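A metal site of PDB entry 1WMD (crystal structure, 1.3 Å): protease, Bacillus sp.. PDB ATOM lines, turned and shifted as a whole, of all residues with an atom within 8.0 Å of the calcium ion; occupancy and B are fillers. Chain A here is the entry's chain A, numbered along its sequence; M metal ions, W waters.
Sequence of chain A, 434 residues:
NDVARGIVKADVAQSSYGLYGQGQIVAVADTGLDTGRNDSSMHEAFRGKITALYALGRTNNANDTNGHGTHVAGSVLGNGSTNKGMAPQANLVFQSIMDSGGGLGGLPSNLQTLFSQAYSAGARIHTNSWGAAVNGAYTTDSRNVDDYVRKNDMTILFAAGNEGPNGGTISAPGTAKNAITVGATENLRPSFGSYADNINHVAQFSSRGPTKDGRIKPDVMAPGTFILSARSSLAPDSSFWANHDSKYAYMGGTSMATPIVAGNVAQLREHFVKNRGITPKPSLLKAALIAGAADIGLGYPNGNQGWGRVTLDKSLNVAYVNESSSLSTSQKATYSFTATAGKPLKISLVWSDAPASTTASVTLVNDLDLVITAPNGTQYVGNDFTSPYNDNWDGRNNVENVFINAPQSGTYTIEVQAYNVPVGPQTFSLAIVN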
ATOM      1  N   VAL A 381     -27.531  21.338   4.776  1.00  0.00           N
ATOM      2  CA  VAL A 381     -26.191  21.837   4.533  1.00  0.00           C
ATOM      3  C   VAL A 381     -26.232  22.846   3.395  1.00  0.00           C
ATOM      4  O   VAL A 381     -27.023  22.703   2.449  1.00  0.00           O
ATOM      5  CB  VAL A 381     -25.313  20.612   4.250  1.00  0.00           C
ATOM      6  CG1 VAL A 381     -23.978  20.919   3.625  1.00  0.00           C
ATOM      7  CG2 VAL A 381     -25.177  19.911   5.623  1.00  0.00           C
ATOM      8  N   ASN A 383     -26.201  24.888   0.208  1.00  0.00           N
ATOM      9  CA  ASN A 383     -26.211  24.602  -1.229  1.00  0.00           C
ATOM     10  C   ASN A 383     -26.540  23.135  -1.586  1.00  0.00           C
ATOM     11  O   ASN A 383     -26.406  22.774  -2.781  1.00  0.00           O
ATOM     12  CB  ASN A 383     -24.931  25.007  -1.939  1.00  0.00           C
ATOM     13  CG  ASN A 383     -24.700  26.516  -1.877  1.00  0.00           C
ATOM     14  OD1 ASN A 383     -25.649  27.264  -1.640  1.00  0.00           O
ATOM     15  ND2 ASN A 383     -23.464  26.957  -2.122  1.00  0.00           N
ATOM     16  N   ASP A 384     -27.027  22.371  -0.607  1.00  0.00           N
ATOM     17  CA  ASP A 384     -27.531  21.038  -0.905  1.00  0.00           C
ATOM     18  C   ASP A 384     -29.030  21.087  -1.193  1.00  0.00           C
ATOM     19  O   ASP A 384     -29.867  21.138  -0.277  1.00  0.00           O
ATOM     20  CB  ASP A 384     -27.251  20.057   0.247  1.00  0.00           C
ATOM     21  CG  ASP A 384     -27.564  18.630  -0.157  1.00  0.00           C
ATOM     22  OD1 ASP A 384     -28.312  18.418  -1.159  1.00  0.00           O
ATOM     23  OD2 ASP A 384     -27.195  17.677   0.564  1.00  0.00           O
ATOM     24  N   PHE A 385     -29.306  20.991  -2.498  1.00  0.00           N
ATOM     25  CA  PHE A 385     -30.721  21.107  -2.891  1.00  0.00           C
ATOM     26  C   PHE A 385     -31.276  19.759  -3.324  1.00  0.00           C
ATOM     27  O   PHE A 385     -32.314  19.744  -3.987  1.00  0.00           O
ATOM     28  CB  PHE A 385     -30.904  22.114  -4.026  1.00  0.00           C
ATOM     29  CG  PHE A 385     -30.675  23.555  -3.601  1.00  0.00           C
ATOM     30  CD1 PHE A 385     -29.414  24.091  -3.620  1.00  0.00           C
ATOM     31  CD2 PHE A 385     -31.755  24.306  -3.172  1.00  0.00           C
ATOM     32  CE1 PHE A 385     -29.223  25.397  -3.199  1.00  0.00           C
ATOM     33  CE2 PHE A 385     -31.591  25.619  -2.741  1.00  0.00           C
ATOM     34  CZ  PHE A 385     -30.288  26.134  -2.740  1.00  0.00           C
ATOM     35  N   THR A 386     -30.606  18.650  -2.949  1.00  0.00           N
ATOM     36  CA  THR A 386     -31.147  17.350  -3.311  1.00  0.00           C
ATOM     37  C   THR A 386     -31.454  16.581  -2.027  1.00  0.00           C
ATOM     38  O   THR A 386     -30.578  16.471  -1.177  1.00  0.00           O
ATOM     39  CB  THR A 386     -30.181  16.520  -4.165  1.00  0.00           C
ATOM     40  OG1 THR A 386     -28.918  16.469  -3.472  1.00  0.00           O
ATOM     41  CG2 THR A 386     -30.045  17.148  -5.554  1.00  0.00           C
ATOM     42  N   SER A 387     -32.649  16.050  -1.888  1.00  0.00           N
ATOM     43  CA  SER A 387     -32.958  15.300  -0.674  1.00  0.00           C
ATOM     44  C   SER A 387     -32.136  14.034  -0.556  1.00  0.00           C
ATOM     45  O   SER A 387     -32.069  13.362  -1.605  1.00  0.00           O
ATOM     46  CB  SER A 387     -34.454  14.883  -0.637  1.00  0.00           C
ATOM     47  OG  SER A 387     -34.727  14.318   0.634  1.00  0.00           O
ATOM     48  N   PRO A 388     -31.547  13.564   0.536  1.00  0.00           N
ATOM     49  CA  PRO A 388     -31.480  14.259   1.813  1.00  0.00           C
ATOM     50  C   PRO A 388     -30.506  15.444   1.749  1.00  0.00           C
ATOM     51  O   PRO A 388     -29.481  15.411   1.080  1.00  0.00           O
ATOM     52  CB  PRO A 388     -30.897  13.227   2.770  1.00  0.00           C
ATOM     53  CG  PRO A 388     -30.239  12.205   1.937  1.00  0.00           C
ATOM     54  CD  PRO A 388     -30.882  12.234   0.591  1.00  0.00           C
ATOM     55  N   TYR A 389     -30.918  16.508   2.476  1.00  0.00           N
ATOM     56  CA  TYR A 389     -30.321  17.819   2.291  1.00  0.00           C
ATOM     57  C   TYR A 389     -29.067  18.036   3.115  1.00  0.00           C
ATOM     58  O   TYR A 389     -28.578  19.158   3.282  1.00  0.00           O
ATOM     59  CB  TYR A 389     -31.361  18.901   2.604  1.00  0.00           C
ATOM     60  CG  TYR A 389     -32.528  18.841   1.623  1.00  0.00           C
ATOM     61  CD1 TYR A 389     -33.774  18.520   2.141  1.00  0.00           C
ATOM     62  CD2 TYR A 389     -32.448  19.103   0.276  1.00  0.00           C
ATOM     63  CE1 TYR A 389     -34.907  18.449   1.337  1.00  0.00           C
ATOM     64  CE2 TYR A 389     -33.558  19.028  -0.573  1.00  0.00           C
ATOM     65  CZ  TYR A 389     -34.783  18.703  -0.024  1.00  0.00           C
ATOM     66  OH  TYR A 389     -35.928  18.612  -0.784  1.00  0.00           O
ATOM     67  N   ASN A 390     -28.540  16.930   3.656  1.00  0.00           N
ATOM     68  CA  ASN A 390     -27.395  17.052   4.538  1.00  0.00           C
ATOM     69  C   ASN A 390     -26.236  16.148   4.119  1.00  0.00           C
ATOM     70  O   ASN A 390     -25.388  15.832   4.941  1.00  0.00           O
ATOM     71  CB  ASN A 390     -27.803  16.762   5.981  1.00  0.00           C
ATOM     72  CG  ASN A 390     -28.197  15.327   6.224  1.00  0.00           C
ATOM     73  OD1 ASN A 390     -28.561  14.592   5.305  1.00  0.00           O
ATOM     74  ND2 ASN A 390     -28.108  14.960   7.514  1.00  0.00           N
ATOM     75  N   ASP A 391     -26.229  15.817   2.817  1.00  0.00           N
ATOM     76  CA  ASP A 391     -25.193  14.858   2.387  1.00  0.00           C
ATOM     77  C   ASP A 391     -24.257  15.462   1.345  1.00  0.00           C
ATOM     78  O   ASP A 391     -23.247  14.784   1.048  1.00  0.00           O
ATOM     79  CB  ASP A 391     -25.749  13.527   1.852  1.00  0.00           C
ATOM     80  CG  ASP A 391     -26.663  13.622   0.666  1.00  0.00           C
ATOM     81  OD1 ASP A 391     -26.790  14.755   0.153  1.00  0.00           O
ATOM     82  OD2 ASP A 391     -27.274  12.607   0.267  1.00  0.00           O
ATOM     83  N   ASN A 392     -24.557  16.644   0.813  1.00  0.00           N
ATOM     84  CA  ASN A 392     -23.665  17.205  -0.213  1.00  0.00           C
ATOM     85  C   ASN A 392     -23.074  18.510   0.297  1.00  0.00           C
ATOM     86  O   ASN A 392     -23.790  19.526   0.404  1.00  0.00           O
ATOM     87  CB  ASN A 392     -24.402  17.484  -1.498  1.00  0.00           C
ATOM     88  CG  ASN A 392     -25.026  16.279  -2.184  1.00  0.00           C
ATOM     89  OD1 ASN A 392     -26.246  16.213  -2.281  1.00  0.00           O
ATOM     90  ND2 ASN A 392     -24.243  15.332  -2.696  1.00  0.00           N
ATOM     91  N   TRP A 393     -21.807  18.489   0.615  1.00  0.00           N
ATOM     92  CA  TRP A 393     -21.127  19.657   1.166  1.00  0.00           C
ATOM     93  C   TRP A 393     -20.386  20.490   0.132  1.00  0.00           C
ATOM     94  O   TRP A 393     -19.831  19.978  -0.855  1.00  0.00           O
ATOM     95  CB  TRP A 393     -20.099  19.200   2.195  1.00  0.00           C
ATOM     96  CG  TRP A 393     -20.705  18.470   3.341  1.00  0.00           C
ATOM     97  CD1 TRP A 393     -21.133  17.188   3.363  1.00  0.00           C
ATOM     98  CD2 TRP A 393     -20.926  19.022   4.646  1.00  0.00           C
ATOM     99  NE1 TRP A 393     -21.628  16.901   4.610  1.00  0.00           N
ATOM    100  CE2 TRP A 393     -21.510  18.001   5.421  1.00  0.00           C
ATOM    101  CE3 TRP A 393     -20.704  20.269   5.232  1.00  0.00           C
ATOM    102  CZ2 TRP A 393     -21.854  18.253   6.761  1.00  0.00           C
ATOM    103  CZ3 TRP A 393     -21.038  20.501   6.548  1.00  0.00           C
ATOM    104  CH2 TRP A 393     -21.618  19.464   7.318  1.00  0.00           C
HETATM  105 CA    CA M   1     -28.323  16.061  -0.991  1.00  0.00          CA
HETATM  106  O   HOH W   1     -28.557  13.804  -1.806  1.00  0.00           O
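Of the 12 residues printed, 5 come within 4 Å of the calcium ion.
The calcium ion is bound by the backbone carbonyl oxygen (O) of Thr 386 (2.3 Å), the side-chain carboxylate (OD1) of Asp 391 (2.3 Å), the side-chain carboxylate (OD1) of Asp 384 (2.4 Å), water W1 (2.4 Å), the side-chain amide oxygen (OD1) of Asn 392 (2.4 Å), the backbone carbonyl oxygen (O) of Pro 388 (2.5 Å), the side-chain carboxylate (OD2) of Asp 384 (2.5 Å) and the side-chain hydroxyl (OG1) of Thr 386 (2.6 Å).
The backbone NH (N) of Asn 390 sits close to the side-chain carboxylate (OD2) of Asp 384 (3.5 Å).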
